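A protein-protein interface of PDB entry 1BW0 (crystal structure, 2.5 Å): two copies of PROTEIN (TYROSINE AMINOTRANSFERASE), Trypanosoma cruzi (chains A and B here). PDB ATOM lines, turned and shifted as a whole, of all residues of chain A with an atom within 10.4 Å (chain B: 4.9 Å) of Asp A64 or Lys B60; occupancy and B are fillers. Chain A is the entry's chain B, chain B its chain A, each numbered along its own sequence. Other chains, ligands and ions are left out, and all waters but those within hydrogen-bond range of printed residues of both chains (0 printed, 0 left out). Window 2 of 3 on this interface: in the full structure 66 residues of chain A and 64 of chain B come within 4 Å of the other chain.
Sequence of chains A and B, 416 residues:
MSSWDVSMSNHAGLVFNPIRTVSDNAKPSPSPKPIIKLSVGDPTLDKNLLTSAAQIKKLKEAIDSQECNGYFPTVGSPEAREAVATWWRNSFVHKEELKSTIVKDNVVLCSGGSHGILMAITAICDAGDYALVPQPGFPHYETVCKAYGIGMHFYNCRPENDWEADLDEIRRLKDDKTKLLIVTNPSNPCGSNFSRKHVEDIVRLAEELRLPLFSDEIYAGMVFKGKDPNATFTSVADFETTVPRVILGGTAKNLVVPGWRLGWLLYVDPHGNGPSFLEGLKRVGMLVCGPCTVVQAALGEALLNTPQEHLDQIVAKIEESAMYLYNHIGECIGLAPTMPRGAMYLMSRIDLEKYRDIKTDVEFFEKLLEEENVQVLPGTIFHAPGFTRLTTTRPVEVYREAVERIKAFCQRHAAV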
ATOM      1  N   ILE A  56     -28.094 -14.363  -0.347  1.00  0.00           N
ATOM      2  CA  ILE A  56     -28.083 -15.315  -1.446  1.00  0.00           C
ATOM      3  C   ILE A  56     -29.279 -15.152  -2.374  1.00  0.00           C
ATOM      4  O   ILE A  56     -29.114 -15.246  -3.596  1.00  0.00           O
ATOM      5  CB  ILE A  56     -28.036 -16.764  -0.932  1.00  0.00           C
ATOM      6  CG1 ILE A  56     -26.761 -17.037  -0.133  1.00  0.00           C
ATOM      7  CG2 ILE A  56     -28.153 -17.758  -2.083  1.00  0.00           C
ATOM      8  CD1 ILE A  56     -26.856 -18.343   0.642  1.00  0.00           C
ATOM      9  N   LYS A  57     -30.480 -14.952  -1.850  1.00  0.00           N
ATOM     10  CA  LYS A  57     -31.672 -14.793  -2.671  1.00  0.00           C
ATOM     11  C   LYS A  57     -31.540 -13.604  -3.617  1.00  0.00           C
ATOM     12  O   LYS A  57     -31.711 -13.725  -4.829  1.00  0.00           O
ATOM     13  CB  LYS A  57     -32.922 -14.603  -1.813  1.00  0.00           C
ATOM     14  CG  LYS A  57     -34.225 -14.590  -2.600  1.00  0.00           C
ATOM     15  CD  LYS A  57     -35.292 -13.820  -1.835  1.00  0.00           C
ATOM     16  CE  LYS A  57     -36.677 -14.059  -2.428  1.00  0.00           C
ATOM     17  NZ  LYS A  57     -37.578 -12.906  -2.124  1.00  0.00           N
ATOM     18  N   LYS A  58     -31.184 -12.448  -3.061  1.00  0.00           N
ATOM     19  CA  LYS A  58     -31.002 -11.237  -3.846  1.00  0.00           C
ATOM     20  C   LYS A  58     -29.883 -11.394  -4.867  1.00  0.00           C
ATOM     21  O   LYS A  58     -29.982 -10.842  -5.965  1.00  0.00           O
ATOM     22  CB  LYS A  58     -30.767 -10.022  -2.949  1.00  0.00           C
ATOM     23  CG  LYS A  58     -30.664  -8.716  -3.720  1.00  0.00           C
ATOM     24  CD  LYS A  58     -31.923  -8.442  -4.537  1.00  0.00           C
ATOM     25  CE  LYS A  58     -31.891  -7.031  -5.110  1.00  0.00           C
ATOM     26  NZ  LYS A  58     -33.260  -6.498  -5.345  1.00  0.00           N
ATOM     27  N   LEU A  59     -28.840 -12.152  -4.542  1.00  0.00           N
ATOM     28  CA  LEU A  59     -27.764 -12.408  -5.485  1.00  0.00           C
ATOM     29  C   LEU A  59     -28.346 -13.109  -6.710  1.00  0.00           C
ATOM     30  O   LEU A  59     -28.223 -12.608  -7.827  1.00  0.00           O
ATOM     31  CB  LEU A  59     -26.629 -13.222  -4.872  1.00  0.00           C
ATOM     32  CG  LEU A  59     -25.404 -13.449  -5.767  1.00  0.00           C
ATOM     33  CD1 LEU A  59     -24.907 -12.149  -6.379  1.00  0.00           C
ATOM     34  CD2 LEU A  59     -24.278 -14.102  -4.982  1.00  0.00           C
ATOM     35  N   LYS A  60     -29.076 -14.201  -6.510  1.00  0.00           N
ATOM     36  CA  LYS A  60     -29.703 -14.925  -7.611  1.00  0.00           C
ATOM     37  C   LYS A  60     -30.689 -14.067  -8.389  1.00  0.00           C
ATOM     38  O   LYS A  60     -30.716 -14.139  -9.621  1.00  0.00           O
ATOM     39  CB  LYS A  60     -30.359 -16.214  -7.107  1.00  0.00           C
ATOM     40  CG  LYS A  60     -29.334 -17.199  -6.557  1.00  0.00           C
ATOM     41  CD  LYS A  60     -29.969 -18.220  -5.628  1.00  0.00           C
ATOM     42  CE  LYS A  60     -30.695 -19.308  -6.404  1.00  0.00           C
ATOM     43  NZ  LYS A  60     -31.366 -20.268  -5.486  1.00  0.00           N
ATOM     44  N   GLU A  61     -31.463 -13.209  -7.727  1.00  0.00           N
ATOM     45  CA  GLU A  61     -32.391 -12.331  -8.420  1.00  0.00           C
ATOM     46  C   GLU A  61     -31.665 -11.317  -9.298  1.00  0.00           C
ATOM     47  O   GLU A  61     -32.122 -10.990 -10.392  1.00  0.00           O
ATOM     48  CB  GLU A  61     -33.266 -11.569  -7.429  1.00  0.00           C
ATOM     49  CG  GLU A  61     -34.072 -12.468  -6.511  1.00  0.00           C
ATOM     50  CD  GLU A  61     -35.168 -11.686  -5.799  1.00  0.00           C
ATOM     51  OE1 GLU A  61     -35.094 -10.433  -5.782  1.00  0.00           O
ATOM     52  OE2 GLU A  61     -36.079 -12.372  -5.279  1.00  0.00           O
ATOM     53  N   ALA A  62     -30.534 -10.804  -8.819  1.00  0.00           N
ATOM     54  CA  ALA A  62     -29.748  -9.842  -9.579  1.00  0.00           C
ATOM     55  C   ALA A  62     -29.177 -10.474 -10.842  1.00  0.00           C
ATOM     56  O   ALA A  62     -29.076  -9.815 -11.879  1.00  0.00           O
ATOM     57  CB  ALA A  62     -28.648  -9.278  -8.695  1.00  0.00           C
ATOM     58  N   ILE A  63     -28.800 -11.741 -10.782  1.00  0.00           N
ATOM     59  CA  ILE A  63     -28.252 -12.472 -11.913  1.00  0.00           C
ATOM     60  C   ILE A  63     -29.302 -12.731 -12.988  1.00  0.00           C
ATOM     61  O   ILE A  63     -29.053 -12.608 -14.188  1.00  0.00           O
ATOM     62  CB  ILE A  63     -27.670 -13.819 -11.428  1.00  0.00           C
ATOM     63  CG1 ILE A  63     -26.510 -13.567 -10.458  1.00  0.00           C
ATOM     64  CG2 ILE A  63     -27.222 -14.696 -12.584  1.00  0.00           C
ATOM     65  CD1 ILE A  63     -26.107 -14.766  -9.634  1.00  0.00           C
ATOM     66  N   ASP A  64     -30.498 -13.118 -12.559  1.00  0.00           N
ATOM     67  CA  ASP A  64     -31.614 -13.436 -13.430  1.00  0.00           C
ATOM     68  C   ASP A  64     -32.151 -12.195 -14.131  1.00  0.00           C
ATOM     69  O   ASP A  64     -32.447 -12.236 -15.325  1.00  0.00           O
ATOM     70  CB  ASP A  64     -32.731 -14.128 -12.638  1.00  0.00           C
ATOM     71  CG  ASP A  64     -32.424 -15.560 -12.258  1.00  0.00           C
ATOM     72  OD1 ASP A  64     -31.593 -16.228 -12.910  1.00  0.00           O
ATOM     73  OD2 ASP A  64     -33.022 -16.065 -11.282  1.00  0.00           O
ATOM     74  N   SER A  65     -32.183 -11.075 -13.424  1.00  0.00           N
ATOM     75  CA  SER A  65     -32.639  -9.806 -13.956  1.00  0.00           C
ATOM     76  C   SER A  65     -31.854  -9.403 -15.201  1.00  0.00           C
ATOM     77  O   SER A  65     -32.362  -8.871 -16.183  1.00  0.00           O
ATOM     78  CB  SER A  65     -32.474  -8.694 -12.914  1.00  0.00           C
ATOM     79  OG  SER A  65     -31.179  -8.112 -12.934  1.00  0.00           O
ATOM     80  N   GLN A  66     -30.537  -9.571 -15.109  1.00  0.00           N
ATOM     81  CA  GLN A  66     -29.599  -9.247 -16.161  1.00  0.00           C
ATOM     82  C   GLN A  66     -29.458  -7.757 -16.412  1.00  0.00           C
ATOM     83  O   GLN A  66     -29.078  -7.333 -17.501  1.00  0.00           O
ATOM     84  CB  GLN A  66     -29.938 -10.030 -17.438  1.00  0.00           C
ATOM     85  CG  GLN A  66     -29.466 -11.478 -17.251  1.00  0.00           C
ATOM     86  CD  GLN A  66     -29.727 -12.296 -18.497  1.00  0.00           C
ATOM     87  OE1 GLN A  66     -28.786 -12.559 -19.250  1.00  0.00           O
ATOM     88  NE2 GLN A  66     -30.994 -12.650 -18.668  1.00  0.00           N
ATOM     89  N   GLU A  67     -29.693  -6.961 -15.373  1.00  0.00           N
ATOM     90  CA  GLU A  67     -29.518  -5.517 -15.488  1.00  0.00           C
ATOM     91  C   GLU A  67     -28.358  -5.090 -14.596  1.00  0.00           C
ATOM     92  O   GLU A  67     -28.023  -3.916 -14.518  1.00  0.00           O
ATOM     93  CB  GLU A  67     -30.806  -4.766 -15.167  1.00  0.00           C
ATOM     94  CG  GLU A  67     -31.682  -4.571 -16.397  1.00  0.00           C
ATOM     95  CD  GLU A  67     -33.168  -4.566 -16.087  1.00  0.00           C
ATOM     96  OE1 GLU A  67     -33.538  -4.413 -14.901  1.00  0.00           O
ATOM     97  OE2 GLU A  67     -33.946  -4.728 -17.062  1.00  0.00           O
ATOM     98  N   CYS A  68     -27.671  -6.076 -14.032  1.00  0.00           N
ATOM     99  CA  CYS A  68     -26.558  -5.852 -13.128  1.00  0.00           C
ATOM    100  C   CYS A  68     -25.232  -6.392 -13.640  1.00  0.00           C
ATOM    101  O   CYS A  68     -24.280  -6.458 -12.854  1.00  0.00           O
ATOM    102  CB  CYS A  68     -26.874  -6.515 -11.775  1.00  0.00           C
ATOM    103  SG  CYS A  68     -28.305  -5.802 -10.933  1.00  0.00           S
ATOM    104  N   ASN A  69     -25.121  -6.726 -14.916  1.00  0.00           N
ATOM    105  CA  ASN A  69     -23.896  -7.267 -15.480  1.00  0.00           C
ATOM    106  C   ASN A  69     -22.974  -6.238 -16.126  1.00  0.00           C
ATOM    107  O   ASN A  69     -21.829  -6.589 -16.446  1.00  0.00           O
ATOM    108  CB  ASN A  69     -24.188  -8.348 -16.537  1.00  0.00           C
ATOM    109  CG  ASN A  69     -25.138  -9.427 -16.053  1.00  0.00           C
ATOM    110  OD1 ASN A  69     -25.073  -9.878 -14.918  1.00  0.00           O
ATOM    111  ND2 ASN A  69     -26.049  -9.854 -16.917  1.00  0.00           N
ATOM    112  N   TRP A 260     -16.208 -13.769  -2.049  1.00  0.00           N
ATOM    113  CA  TRP A 260     -16.988 -12.889  -2.912  1.00  0.00           C
ATOM    114  C   TRP A 260     -16.262 -11.584  -3.189  1.00  0.00           C
ATOM    115  O   TRP A 260     -16.717 -10.826  -4.029  1.00  0.00           O
ATOM    116  CB  TRP A 260     -18.381 -12.637  -2.323  1.00  0.00           C
ATOM    117  CG  TRP A 260     -19.269 -13.848  -2.295  1.00  0.00           C
ATOM    118  CD1 TRP A 260     -18.906 -15.162  -2.461  1.00  0.00           C
ATOM    119  CD2 TRP A 260     -20.682 -13.860  -2.052  1.00  0.00           C
ATOM    120  NE1 TRP A 260     -20.000 -15.978  -2.367  1.00  0.00           N
ATOM    121  CE2 TRP A 260     -21.107 -15.201  -2.111  1.00  0.00           C
ATOM    122  CE3 TRP A 260     -21.632 -12.869  -1.807  1.00  0.00           C
ATOM    123  CZ2 TRP A 260     -22.438 -15.574  -1.934  1.00  0.00           C
ATOM    124  CZ3 TRP A 260     -22.952 -13.236  -1.641  1.00  0.00           C
ATOM    125  CH2 TRP A 260     -23.342 -14.579  -1.694  1.00  0.00           C
ATOM    126  N   VAL A 294     -22.520  -7.887  -9.639  1.00  0.00           N
ATOM    127  CA  VAL A 294     -23.609  -8.764  -9.197  1.00  0.00           C
ATOM    128  C   VAL A 294     -23.587  -8.888  -7.683  1.00  0.00           C
ATOM    129  O   VAL A 294     -24.629  -8.866  -7.016  1.00  0.00           O
ATOM    130  CB  VAL A 294     -23.498 -10.051 -10.023  1.00  0.00           C
ATOM    131  CG1 VAL A 294     -23.036 -11.265  -9.245  1.00  0.00           C
ATOM    132  CG2 VAL A 294     -24.811 -10.301 -10.757  1.00  0.00           C
ATOM    133  N   ALA A 297     -24.847  -5.515  -6.138  1.00  0.00           N
ATOM    134  CA  ALA A 297     -26.284  -5.439  -6.286  1.00  0.00           C
ATOM    135  C   ALA A 297     -27.040  -6.211  -5.213  1.00  0.00           C
ATOM    136  O   ALA A 297     -28.234  -5.965  -5.029  1.00  0.00           O
ATOM    137  CB  ALA A 297     -26.676  -5.981  -7.660  1.00  0.00           C
ATOM    138  N   ILE B  56     -25.091 -18.483 -16.587  1.00  0.00           N
ATOM    139  CA  ILE B  56     -26.070 -18.106 -15.577  1.00  0.00           C
ATOM    140  C   ILE B  56     -26.404 -19.286 -14.674  1.00  0.00           C
ATOM    141  O   ILE B  56     -26.353 -19.124 -13.453  1.00  0.00           O
ATOM    142  CB  ILE B  56     -27.365 -17.518 -16.157  1.00  0.00           C
ATOM    143  CG1 ILE B  56     -27.100 -16.088 -16.658  1.00  0.00           C
ATOM    144  CG2 ILE B  56     -28.495 -17.509 -15.135  1.00  0.00           C
ATOM    145  CD1 ILE B  56     -28.259 -15.488 -17.432  1.00  0.00           C
ATOM    146  N   LYS B  57     -26.751 -20.425 -15.258  1.00  0.00           N
ATOM    147  CA  LYS B  57     -27.116 -21.599 -14.476  1.00  0.00           C
ATOM    148  C   LYS B  57     -26.026 -22.064 -13.520  1.00  0.00           C
ATOM    149  O   LYS B  57     -26.311 -22.273 -12.335  1.00  0.00           O
ATOM    150  CB  LYS B  57     -27.524 -22.751 -15.395  1.00  0.00           C
ATOM    151  CG  LYS B  57     -28.360 -23.810 -14.698  1.00  0.00           C
ATOM    152  CD  LYS B  57     -28.205 -25.158 -15.393  1.00  0.00           C
ATOM    153  CE  LYS B  57     -28.951 -26.240 -14.615  1.00  0.00           C
ATOM    154  NZ  LYS B  57     -28.780 -27.571 -15.268  1.00  0.00           N
ATOM    155  N   LYS B  58     -24.794 -22.237 -14.000  1.00  0.00           N
ATOM    156  CA  LYS B  58     -23.714 -22.665 -13.120  1.00  0.00           C
ATOM    157  C   LYS B  58     -23.464 -21.655 -12.005  1.00  0.00           C
ATOM    158  O   LYS B  58     -23.336 -22.058 -10.849  1.00  0.00           O
ATOM    159  CB  LYS B  58     -22.424 -22.956 -13.880  1.00  0.00           C
ATOM    160  CG  LYS B  58     -21.273 -23.440 -13.013  1.00  0.00           C
ATOM    161  CD  LYS B  58     -21.654 -24.661 -12.195  1.00  0.00           C
ATOM    162  CE  LYS B  58     -20.422 -25.433 -11.754  1.00  0.00           C
ATOM    163  NZ  LYS B  58     -20.792 -26.467 -10.740  1.00  0.00           N
ATOM    164  N   LEU B  59     -23.428 -20.360 -12.312  1.00  0.00           N
ATOM    165  CA  LEU B  59     -23.250 -19.348 -11.274  1.00  0.00           C
ATOM    166  C   LEU B  59     -24.295 -19.535 -10.181  1.00  0.00           C
ATOM    167  O   LEU B  59     -23.899 -19.611  -9.017  1.00  0.00           O
ATOM    168  CB  LEU B  59     -23.272 -17.916 -11.808  1.00  0.00           C
ATOM    169  CG  LEU B  59     -23.067 -16.791 -10.790  1.00  0.00           C
ATOM    170  CD1 LEU B  59     -21.794 -17.006  -9.984  1.00  0.00           C
ATOM    171  CD2 LEU B  59     -23.021 -15.428 -11.469  1.00  0.00           C
ATOM    172  N   LYS B  60     -25.578 -19.678 -10.503  1.00  0.00           N
ATOM    173  CA  LYS B  60     -26.592 -19.904  -9.479  1.00  0.00           C
ATOM    174  C   LYS B  60     -26.359 -21.174  -8.670  1.00  0.00           C
ATOM    175  O   LYS B  60     -26.618 -21.162  -7.456  1.00  0.00           O
ATOM    176  CB  LYS B  60     -28.005 -19.888 -10.062  1.00  0.00           C
ATOM    177  CG  LYS B  60     -28.484 -18.483 -10.407  1.00  0.00           C
ATOM    178  CD  LYS B  60     -29.988 -18.399 -10.564  1.00  0.00           C
ATOM    179  CE  LYS B  60     -30.490 -19.066 -11.828  1.00  0.00           C
ATOM    180  NZ  LYS B  60     -31.981 -19.064 -11.901  1.00  0.00           N
ATOM    181  N   GLU B  61     -25.857 -22.250  -9.266  1.00  0.00           N
ATOM    182  CA  GLU B  61     -25.596 -23.484  -8.543  1.00  0.00           C
ATOM    183  C   GLU B  61     -24.397 -23.390  -7.601  1.00  0.00           C
ATOM    184  O   GLU B  61     -24.385 -24.040  -6.548  1.00  0.00           O
ATOM    185  CB  GLU B  61     -25.350 -24.653  -9.492  1.00  0.00           C
ATOM    186  CG  GLU B  61     -26.591 -25.173 -10.204  1.00  0.00           C
ATOM    187  CD  GLU B  61     -26.161 -26.137 -11.308  1.00  0.00           C
ATOM    188  OE1 GLU B  61     -25.157 -26.855 -11.085  1.00  0.00           O
ATOM    189  OE2 GLU B  61     -26.815 -26.134 -12.372  1.00  0.00           O
ATOM    190  N   ALA B  62     -23.384 -22.608  -7.979  1.00  0.00           N
ATOM    191  CA  ALA B  62     -22.209 -22.441  -7.131  1.00  0.00           C
ATOM    192  C   ALA B  62     -22.604 -21.678  -5.870  1.00  0.00           C
ATOM    193  O   ALA B  62     -22.181 -21.998  -4.762  1.00  0.00           O
ATOM    194  CB  ALA B  62     -21.108 -21.756  -7.907  1.00  0.00           C
ATOM    195  N   ILE B  63     -23.492 -20.705  -6.011  1.00  0.00           N
ATOM    196  CA  ILE B  63     -24.063 -19.946  -4.918  1.00  0.00           C
ATOM    197  C   ILE B  63     -24.933 -20.833  -4.037  1.00  0.00           C
ATOM    198  O   ILE B  63     -24.809 -20.810  -2.812  1.00  0.00           O
ATOM    199  CB  ILE B  63     -24.901 -18.775  -5.473  1.00  0.00           C
ATOM    200  CG1 ILE B  63     -24.004 -17.844  -6.294  1.00  0.00           C
ATOM    201  CG2 ILE B  63     -25.588 -18.013  -4.355  1.00  0.00           C
ATOM    202  CD1 ILE B  63     -24.740 -16.789  -7.087  1.00  0.00           C
ATOM    203  N   ASP B  64     -25.806 -21.640  -4.637  1.00  0.00           N
ATOM    204  CA  ASP B  64     -26.681 -22.521  -3.871  1.00  0.00           C
ATOM    205  C   ASP B  64     -25.926 -23.626  -3.153  1.00  0.00           C
ATOM    206  O   ASP B  64     -26.337 -24.032  -2.069  1.00  0.00           O
ATOM    207  CB  ASP B  64     -27.789 -23.107  -4.748  1.00  0.00           C
ATOM    208  CG  ASP B  64     -29.010 -22.225  -4.905  1.00  0.00           C
ATOM    209  OD1 ASP B  64     -29.179 -21.238  -4.151  1.00  0.00           O
ATOM    210  OD2 ASP B  64     -29.846 -22.507  -5.799  1.00  0.00           O
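Of the printed residues of chain B, Ile A56 touches Ile B63. Printed residues of chain B within 4 Å of Leu A59: Ile B63. Of the printed residues of chain B, Ile A63 touches Leu B59 (3.7 Å) and Ile B63 (3.5 Å). Asp A64 touches just one residue of chain B: Lys B60. Of the printed residues of chain B, Gln A66 touches Ile B56 (3.5 Å). Val A294 touches none of the printed residues of chain B. Ala A297 touches none of the printed residues of chain B. Of the printed residues of chain A, Ile B56 touches Gln A66. Leu B59 touches just one residue of chain A: Ile A63. Lys B60 touches just one residue of chain A: Asp A64. No residue of chain A comes within 4 Å of Glu B61. No residue of chain A comes within 4 Å of Ala B62. Of the printed residues of chain A, Ile B63 touches Ile A56, Leu A59 and Ile A63. Asp B64 touches just one residue of chain A: Lys A60 (2.7 Å). The nearest residue of chain B that does not touch Asp A64 is Ile B56 (4.02 Å).
Of the 17 printed residues of chain A, 6 touch a printed residue of chain B. Printed residues of chain A that touch a printed residue of chain B: Ile A56, Leu A59, Lys A60, Ile A63, Asp A64 and Gln A66. Hydrophobic or aromatic side chains of chain A that line the printed part of chain B: Ile A56, Leu A59 and Ile A63. Along chain A the printed residues that touch a printed residue of chain B span positions 56 to 66. Hydrophobic or aromatic side chains of chain B within 4 Å of the printed part of chain A: Ile B56, Leu B59 and Ile B63. Among the printed residues, Asp or Glu carboxylates within 4 Å of a Lys or Arg side-chain nitrogen of the other chain: Lys A60 with Asp B64 and Asp A64 with Lys B60.
Among the printed residues, merely in contact across the chains: Ile A56 with Ile B63, Leu A59 with Ile B63, Gln A66 with Ile B56, Ile A63 with Ile B63 and Ile A63 with Leu B59.
Ile A56 touches Ile B63, but with the chains exchanged Ile A63 does not touch Ile B56 (4.01 Å). Leu A59 touches Ile B63, and with the chains exchanged Ile A63 touches Leu B59. Lys A60 touches Asp B64, and with the chains exchanged Asp A64 touches Lys B60. Ile A63 touches its own counterpart, Ile B63.
The side-chain amino group (NZ) of Lys B60 is in salt-bridge range of the side-chain carboxylate (OD1) of Asp A64 (3.0 Å). NZ of Lys A60 is in salt-bridge range of OD2 of Asp B64.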
